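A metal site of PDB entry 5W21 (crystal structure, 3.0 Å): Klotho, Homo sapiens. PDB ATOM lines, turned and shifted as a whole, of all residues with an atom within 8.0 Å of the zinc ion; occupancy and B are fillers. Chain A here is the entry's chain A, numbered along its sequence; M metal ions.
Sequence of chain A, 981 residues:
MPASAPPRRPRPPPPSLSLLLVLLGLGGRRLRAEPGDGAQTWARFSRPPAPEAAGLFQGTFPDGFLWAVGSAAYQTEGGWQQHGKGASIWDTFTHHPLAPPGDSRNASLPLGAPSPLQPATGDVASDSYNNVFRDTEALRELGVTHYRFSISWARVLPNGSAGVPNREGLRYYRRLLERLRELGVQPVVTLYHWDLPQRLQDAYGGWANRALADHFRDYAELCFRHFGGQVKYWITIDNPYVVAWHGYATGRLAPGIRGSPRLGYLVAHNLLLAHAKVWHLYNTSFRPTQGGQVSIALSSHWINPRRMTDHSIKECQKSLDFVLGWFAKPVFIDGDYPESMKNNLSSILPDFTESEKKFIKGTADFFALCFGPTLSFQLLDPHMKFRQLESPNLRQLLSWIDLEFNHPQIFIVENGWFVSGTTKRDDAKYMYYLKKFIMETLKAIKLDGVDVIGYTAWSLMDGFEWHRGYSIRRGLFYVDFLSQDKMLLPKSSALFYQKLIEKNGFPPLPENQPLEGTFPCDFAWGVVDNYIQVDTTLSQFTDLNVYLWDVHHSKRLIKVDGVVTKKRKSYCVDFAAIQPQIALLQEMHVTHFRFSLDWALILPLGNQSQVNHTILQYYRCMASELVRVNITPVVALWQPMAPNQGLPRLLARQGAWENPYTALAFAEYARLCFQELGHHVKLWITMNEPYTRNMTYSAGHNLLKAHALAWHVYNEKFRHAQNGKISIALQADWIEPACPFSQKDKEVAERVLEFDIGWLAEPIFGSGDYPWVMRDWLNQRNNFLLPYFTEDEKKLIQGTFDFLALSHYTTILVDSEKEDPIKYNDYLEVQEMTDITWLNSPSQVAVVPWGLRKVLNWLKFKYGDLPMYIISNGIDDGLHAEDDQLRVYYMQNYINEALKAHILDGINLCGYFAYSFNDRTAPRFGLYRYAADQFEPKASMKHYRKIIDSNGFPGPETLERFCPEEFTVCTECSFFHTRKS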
ATOM      1  N   ARG A 425      17.659   3.084  17.938  1.00  0.00           N
ATOM      2  CA  ARG A 425      17.340   1.920  17.123  1.00  0.00           C
ATOM      3  C   ARG A 425      17.575   0.608  17.854  1.00  0.00           C
ATOM      4  O   ARG A 425      17.036  -0.427  17.434  1.00  0.00           O
ATOM      5  CB  ARG A 425      18.153   1.942  15.825  1.00  0.00           C
ATOM      6  CG  ARG A 425      17.774   3.085  14.895  1.00  0.00           C
ATOM      7  CD  ARG A 425      18.502   2.979  13.562  1.00  0.00           C
ATOM      8  NE  ARG A 425      18.205   1.718  12.873  1.00  0.00           N
ATOM      9  CZ  ARG A 425      18.592   1.439  11.633  1.00  0.00           C
ATOM     10  NH1 ARG A 425      19.290   2.337  10.930  1.00  0.00           N
ATOM     11  NH2 ARG A 425      18.282   0.276  11.091  1.00  0.00           N
ATOM     12  N   ASP A 426      18.357   0.608  18.930  1.00  0.00           N
ATOM     13  CA  ASP A 426      18.643  -0.597  19.705  1.00  0.00           C
ATOM     14  C   ASP A 426      17.720  -0.604  20.918  1.00  0.00           C
ATOM     15  O   ASP A 426      17.950   0.134  21.885  1.00  0.00           O
ATOM     16  CB  ASP A 426      20.105  -0.643  20.112  1.00  0.00           C
ATOM     17  CG  ASP A 426      20.420  -1.808  21.037  1.00  0.00           C
ATOM     18  OD1 ASP A 426      20.514  -2.949  20.550  1.00  0.00           O
ATOM     19  OD2 ASP A 426      20.548  -1.574  22.259  1.00  0.00           O
ATOM     20  N   ASP A 427      16.678  -1.442  20.877  1.00  0.00           N
ATOM     21  CA  ASP A 427      15.672  -1.514  21.936  1.00  0.00           C
ATOM     22  C   ASP A 427      15.467  -2.984  22.312  1.00  0.00           C
ATOM     23  O   ASP A 427      14.414  -3.585  22.047  1.00  0.00           O
ATOM     24  CB  ASP A 427      14.363  -0.853  21.497  1.00  0.00           C
ATOM     25  CG  ASP A 427      13.847  -1.400  20.170  1.00  0.00           C
ATOM     26  OD1 ASP A 427      14.659  -1.897  19.378  1.00  0.00           O
ATOM     27  OD2 ASP A 427      12.624  -1.322  19.933  1.00  0.00           O
ATOM     28  N   ALA A 428      16.477  -3.564  22.966  1.00  0.00           N
ATOM     29  CA  ALA A 428      16.381  -4.962  23.376  1.00  0.00           C
ATOM     30  C   ALA A 428      15.297  -5.165  24.413  1.00  0.00           C
ATOM     31  O   ALA A 428      14.584  -6.180  24.387  1.00  0.00           O
ATOM     32  CB  ALA A 428      17.724  -5.453  23.905  1.00  0.00           C
ATOM     33  N   LYS A 429      15.144  -4.217  25.342  1.00  0.00           N
ATOM     34  CA  LYS A 429      14.109  -4.316  26.359  1.00  0.00           C
ATOM     35  C   LYS A 429      12.730  -4.502  25.731  1.00  0.00           C
ATOM     36  O   LYS A 429      11.948  -5.349  26.164  1.00  0.00           O
ATOM     37  CB  LYS A 429      14.134  -3.077  27.252  1.00  0.00           C
ATOM     38  CG  LYS A 429      12.997  -2.982  28.250  1.00  0.00           C
ATOM     39  CD  LYS A 429      13.064  -1.654  28.984  1.00  0.00           C
ATOM     40  CE  LYS A 429      11.871  -1.447  29.897  1.00  0.00           C
ATOM     41  NZ  LYS A 429      11.902  -0.098  30.527  1.00  0.00           N
ATOM     42  N   MET A 431      12.037  -5.617  22.655  1.00  0.00           N
ATOM     43  CA  MET A 431      11.899  -6.807  21.819  1.00  0.00           C
ATOM     44  C   MET A 431      11.733  -8.061  22.661  1.00  0.00           C
ATOM     45  O   MET A 431      11.098  -9.023  22.202  1.00  0.00           O
ATOM     46  CB  MET A 431      13.097  -6.943  20.873  1.00  0.00           C
ATOM     47  CG  MET A 431      14.384  -7.447  21.514  1.00  0.00           C
ATOM     48  SD  MET A 431      15.661  -7.755  20.277  1.00  0.00           S
ATOM     49  CE  MET A 431      14.981  -9.182  19.436  1.00  0.00           C
ATOM     50  N   TYR A 432      12.262  -8.080  23.881  1.00  0.00           N
ATOM     51  CA  TYR A 432      12.067  -9.242  24.740  1.00  0.00           C
ATOM     52  C   TYR A 432      10.723  -9.175  25.460  1.00  0.00           C
ATOM     53  O   TYR A 432      10.140 -10.228  25.758  1.00  0.00           O
ATOM     54  CB  TYR A 432      13.216  -9.367  25.736  1.00  0.00           C
ATOM     55  CG  TYR A 432      14.500  -9.862  25.088  1.00  0.00           C
ATOM     56  CD1 TYR A 432      15.495  -8.963  24.721  1.00  0.00           C
ATOM     57  CD2 TYR A 432      14.701 -11.211  24.827  1.00  0.00           C
ATOM     58  CE1 TYR A 432      16.659  -9.406  24.120  1.00  0.00           C
ATOM     59  CE2 TYR A 432      15.863 -11.656  24.236  1.00  0.00           C
ATOM     60  CZ  TYR A 432      16.839 -10.746  23.878  1.00  0.00           C
ATOM     61  OH  TYR A 432      18.002 -11.191  23.287  1.00  0.00           O
ATOM     62  N   SER A 492      15.554  -3.232  16.445  1.00  0.00           N
ATOM     63  CA  SER A 492      15.827  -4.653  16.623  1.00  0.00           C
ATOM     64  C   SER A 492      14.535  -5.451  16.773  1.00  0.00           C
ATOM     65  O   SER A 492      14.424  -6.560  16.253  1.00  0.00           O
ATOM     66  CB  SER A 492      16.724  -4.869  17.840  1.00  0.00           C
ATOM     67  OG  SER A 492      17.940  -4.152  17.711  1.00  0.00           O
ATOM     68  N   PRO A 737      25.049 -11.767  23.362  1.00  0.00           N
ATOM     69  CA  PRO A 737      24.541 -10.434  22.990  1.00  0.00           C
ATOM     70  C   PRO A 737      23.021 -10.413  22.975  1.00  0.00           C
ATOM     71  O   PRO A 737      22.366 -11.329  22.473  1.00  0.00           O
ATOM     72  CB  PRO A 737      25.120 -10.214  21.591  1.00  0.00           C
ATOM     73  CG  PRO A 737      26.288 -11.137  21.507  1.00  0.00           C
ATOM     74  CD  PRO A 737      25.917 -12.342  22.330  1.00  0.00           C
ATOM     75  N   ALA A 738      22.452  -9.339  23.530  1.00  0.00           N
ATOM     76  CA  ALA A 738      21.002  -9.164  23.532  1.00  0.00           C
ATOM     77  C   ALA A 738      20.463  -9.172  22.106  1.00  0.00           C
ATOM     78  O   ALA A 738      19.639 -10.022  21.741  1.00  0.00           O
ATOM     79  CB  ALA A 738      20.628  -7.875  24.252  1.00  0.00           C
ATOM     80  N   CYS A 739      20.908  -8.225  21.283  1.00  0.00           N
ATOM     81  CA  CYS A 739      20.582  -8.220  19.871  1.00  0.00           C
ATOM     82  C   CYS A 739      21.599  -9.081  19.145  1.00  0.00           C
ATOM     83  O   CYS A 739      22.774  -8.692  19.054  1.00  0.00           O
ATOM     84  CB  CYS A 739      20.586  -6.797  19.328  1.00  0.00           C
ATOM     85  SG  CYS A 739      19.686  -5.609  20.340  1.00  0.00           S
ATOM     86  N   PRO A 740      21.215 -10.251  18.621  1.00  0.00           N
ATOM     87  CA  PRO A 740      22.206 -11.169  18.043  1.00  0.00           C
ATOM     88  C   PRO A 740      22.855 -10.654  16.759  1.00  0.00           C
ATOM     89  O   PRO A 740      23.784 -11.297  16.271  1.00  0.00           O
ATOM     90  CB  PRO A 740      21.400 -12.445  17.784  1.00  0.00           C
ATOM     91  CG  PRO A 740      19.996 -11.957  17.610  1.00  0.00           C
ATOM     92  CD  PRO A 740      19.846 -10.789  18.532  1.00  0.00           C
ATOM     93  N   PHE A 741      22.388  -9.538  16.204  1.00  0.00           N
ATOM     94  CA  PHE A 741      22.944  -8.986  14.978  1.00  0.00           C
ATOM     95  C   PHE A 741      23.631  -7.654  15.192  1.00  0.00           C
ATOM     96  O   PHE A 741      24.187  -7.100  14.236  1.00  0.00           O
ATOM     97  CB  PHE A 741      21.846  -8.841  13.922  1.00  0.00           C
ATOM     98  CG  PHE A 741      21.135 -10.135  13.609  1.00  0.00           C
ATOM     99  CD1 PHE A 741      19.954 -10.465  14.266  1.00  0.00           C
ATOM    100  CD2 PHE A 741      21.643 -11.018  12.676  1.00  0.00           C
ATOM    101  CE1 PHE A 741      19.296 -11.648  13.989  1.00  0.00           C
ATOM    102  CE2 PHE A 741      20.996 -12.200  12.391  1.00  0.00           C
ATOM    103  CZ  PHE A 741      19.818 -12.511  13.053  1.00  0.00           C
ATOM    104  N   SER A 742      23.621  -7.110  16.407  1.00  0.00           N
ATOM    105  CA  SER A 742      24.262  -5.831  16.685  1.00  0.00           C
ATOM    106  C   SER A 742      25.747  -6.040  16.950  1.00  0.00           C
ATOM    107  O   SER A 742      26.141  -6.933  17.715  1.00  0.00           O
ATOM    108  CB  SER A 742      23.593  -5.154  17.876  1.00  0.00           C
ATOM    109  OG  SER A 742      24.156  -3.878  18.120  1.00  0.00           O
ATOM    110  N   GLN A 743      26.590  -5.218  16.312  1.00  0.00           N
ATOM    111  CA  GLN A 743      28.024  -5.333  16.520  1.00  0.00           C
ATOM    112  C   GLN A 743      28.423  -4.907  17.924  1.00  0.00           C
ATOM    113  O   GLN A 743      29.239  -5.577  18.568  1.00  0.00           O
ATOM    114  CB  GLN A 743      28.773  -4.497  15.476  1.00  0.00           C
ATOM    115  CG  GLN A 743      28.702  -5.053  14.068  1.00  0.00           C
ATOM    116  CD  GLN A 743      29.456  -6.357  13.911  1.00  0.00           C
ATOM    117  OE1 GLN A 743      30.360  -6.666  14.689  1.00  0.00           O
ATOM    118  NE2 GLN A 743      29.071  -7.141  12.909  1.00  0.00           N
ATOM    119  N   LYS A 744      27.854  -3.808  18.423  1.00  0.00           N
ATOM    120  CA  LYS A 744      28.221  -3.316  19.745  1.00  0.00           C
ATOM    121  C   LYS A 744      27.832  -4.306  20.826  1.00  0.00           C
ATOM    122  O   LYS A 744      28.568  -4.484  21.809  1.00  0.00           O
ATOM    123  CB  LYS A 744      27.586  -1.947  19.998  1.00  0.00           C
ATOM    124  CG  LYS A 744      28.104  -0.857  19.076  1.00  0.00           C
ATOM    125  CD  LYS A 744      27.467   0.482  19.405  1.00  0.00           C
ATOM    126  CE  LYS A 744      27.986   1.582  18.485  1.00  0.00           C
ATOM    127  NZ  LYS A 744      29.452   1.758  18.603  1.00  0.00           N
ATOM    128  N   ASP A 745      26.686  -4.959  20.680  1.00  0.00           N
ATOM    129  CA  ASP A 745      26.295  -5.989  21.636  1.00  0.00           C
ATOM    130  C   ASP A 745      27.247  -7.171  21.602  1.00  0.00           C
ATOM    131  O   ASP A 745      27.483  -7.814  22.633  1.00  0.00           O
ATOM    132  CB  ASP A 745      24.866  -6.445  21.381  1.00  0.00           C
ATOM    133  CG  ASP A 745      23.847  -5.352  21.623  1.00  0.00           C
ATOM    134  OD1 ASP A 745      24.241  -4.235  21.990  1.00  0.00           O
ATOM    135  OD2 ASP A 745      22.639  -5.623  21.437  1.00  0.00           O
ATOM    136  N   LYS A 746      27.803  -7.487  20.431  1.00  0.00           N
ATOM    137  CA  LYS A 746      28.719  -8.616  20.331  1.00  0.00           C
ATOM    138  C   LYS A 746      30.067  -8.284  20.970  1.00  0.00           C
ATOM    139  O   LYS A 746      30.695  -9.151  21.578  1.00  0.00           O
ATOM    140  CB  LYS A 746      28.889  -9.020  18.872  1.00  0.00           C
ATOM    141  CG  LYS A 746      28.565 -10.484  18.607  1.00  0.00           C
ATOM    142  CD  LYS A 746      29.344 -11.400  19.528  1.00  0.00           C
ATOM    143  CE  LYS A 746      28.895 -12.846  19.405  1.00  0.00           C
ATOM    144  NZ  LYS A 746      29.581 -13.724  20.384  1.00  0.00           N
ATOM    145  N   VAL A 748      30.630  -5.974  23.406  1.00  0.00           N
ATOM    146  CA  VAL A 748      30.496  -5.894  24.852  1.00  0.00           C
ATOM    147  C   VAL A 748      30.289  -7.277  25.448  1.00  0.00           C
ATOM    148  O   VAL A 748      30.607  -7.520  26.622  1.00  0.00           O
ATOM    149  CB  VAL A 748      29.357  -4.936  25.262  1.00  0.00           C
ATOM    150  CG1 VAL A 748      29.586  -3.554  24.659  1.00  0.00           C
ATOM    151  CG2 VAL A 748      28.011  -5.497  24.858  1.00  0.00           C
ATOM    152  N   VAL A 814      23.537  -9.327  27.381  1.00  0.00           N
ATOM    153  CA  VAL A 814      24.266  -8.065  27.491  1.00  0.00           C
ATOM    154  C   VAL A 814      23.890  -7.163  26.325  1.00  0.00           C
ATOM    155  O   VAL A 814      23.750  -7.627  25.189  1.00  0.00           O
ATOM    156  CB  VAL A 814      25.794  -8.294  27.539  1.00  0.00           C
ATOM    157  CG1 VAL A 814      26.194  -9.011  28.817  1.00  0.00           C
ATOM    158  CG2 VAL A 814      26.246  -9.085  26.318  1.00  0.00           C
ATOM    159  N   ASP A 815      23.749  -5.870  26.613  1.00  0.00           N
ATOM    160  CA  ASP A 815      23.407  -4.878  25.609  1.00  0.00           C
ATOM    161  C   ASP A 815      24.275  -3.645  25.805  1.00  0.00           C
ATOM    162  O   ASP A 815      24.632  -3.300  26.944  1.00  0.00           O
ATOM    163  CB  ASP A 815      21.921  -4.502  25.656  1.00  0.00           C
ATOM    164  CG  ASP A 815      21.502  -3.591  24.517  1.00  0.00           C
ATOM    165  OD1 ASP A 815      21.981  -2.434  24.459  1.00  0.00           O
ATOM    166  OD2 ASP A 815      20.703  -4.024  23.665  1.00  0.00           O
ATOM    167  N   SER A 816      24.610  -2.985  24.697  1.00  0.00           N
ATOM    168  CA  SER A 816      25.550  -1.872  24.728  1.00  0.00           C
ATOM    169  C   SER A 816      24.894  -0.572  25.170  1.00  0.00           C
ATOM    170  O   SER A 816      25.515   0.217  25.895  1.00  0.00           O
ATOM    171  CB  SER A 816      26.200  -1.699  23.359  1.00  0.00           C
ATOM    172  OG  SER A 816      25.226  -1.409  22.369  1.00  0.00           O
ATOM    173  N   GLU A 817      23.656  -0.320  24.754  1.00  0.00           N
ATOM    174  CA  GLU A 817      23.005   0.950  25.033  1.00  0.00           C
ATOM    175  C   GLU A 817      22.523   1.009  26.474  1.00  0.00           C
ATOM    176  O   GLU A 817      22.040   0.012  27.030  1.00  0.00           O
ATOM    177  CB  GLU A 817      21.834   1.170  24.079  1.00  0.00           C
ATOM    178  CG  GLU A 817      22.241   1.200  22.607  1.00  0.00           C
ATOM    179  CD  GLU A 817      23.214   2.330  22.283  1.00  0.00           C
ATOM    180  OE1 GLU A 817      23.148   3.379  22.949  1.00  0.00           O
ATOM    181  OE2 GLU A 817      24.036   2.147  21.362  1.00  0.00           O
ATOM    182  N   GLN A 831      24.620  -3.165  29.703  1.00  0.00           N
ATOM    183  CA  GLN A 831      23.305  -3.340  30.305  1.00  0.00           C
ATOM    184  C   GLN A 831      23.037  -4.835  30.405  1.00  0.00           C
ATOM    185  O   GLN A 831      22.863  -5.511  29.379  1.00  0.00           O
ATOM    186  CB  GLN A 831      22.230  -2.636  29.485  1.00  0.00           C
ATOM    187  CG  GLN A 831      20.852  -2.659  30.126  1.00  0.00           C
ATOM    188  CD  GLN A 831      20.781  -1.806  31.377  1.00  0.00           C
ATOM    189  OE1 GLN A 831      21.021  -0.595  31.338  1.00  0.00           O
ATOM    190  NE2 GLN A 831      20.459  -2.432  32.507  1.00  0.00           N
ATOM    191  N   MET A 833      20.932  -8.061  31.040  1.00  0.00           N
ATOM    192  CA  MET A 833      19.531  -8.402  30.849  1.00  0.00           C
ATOM    193  C   MET A 833      19.378  -9.917  30.899  1.00  0.00           C
ATOM    194  O   MET A 833      20.333 -10.657  31.120  1.00  0.00           O
ATOM    195  CB  MET A 833      19.002  -7.852  29.510  1.00  0.00           C
ATOM    196  CG  MET A 833      19.281  -6.370  29.294  1.00  0.00           C
ATOM    197  SD  MET A 833      18.832  -5.798  27.640  1.00  0.00           S
ATOM    198  CE  MET A 833      17.096  -6.249  27.580  1.00  0.00           C
HETATM  199 ZN    ZN M   1      21.075  -4.445  21.753  1.00  0.00          ZN
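The side-chain carboxylate (OD1) of Asp 745 sits at hydrogen-bond distance from the backbone NH (N) of Ser 816. The side-chain carboxylate of Asp 815 is in hydrogen-bond range of the backbone NH of Glu 817, 2.7 Å away. O of Asp 815 lies within hydrogen-bond range of N of Gln 831 (2.8 Å). SG of Cys 739 lies close to OG of Ser 492, 3.5 Å away.
Of the 25 residues printed, 4 come within 4 Å of the zinc ion.
The zinc ion is bound by OD2 of Asp 745. The zinc ion is bound by OD2 of Asp 815 (2.0 Å). The side-chain carboxylate (OD1) of Asp 426 binds the zinc ion (2.0 Å). The side-chain sulfur (SG) of Cys 739 binds the zinc ion, at 2.3 Å.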
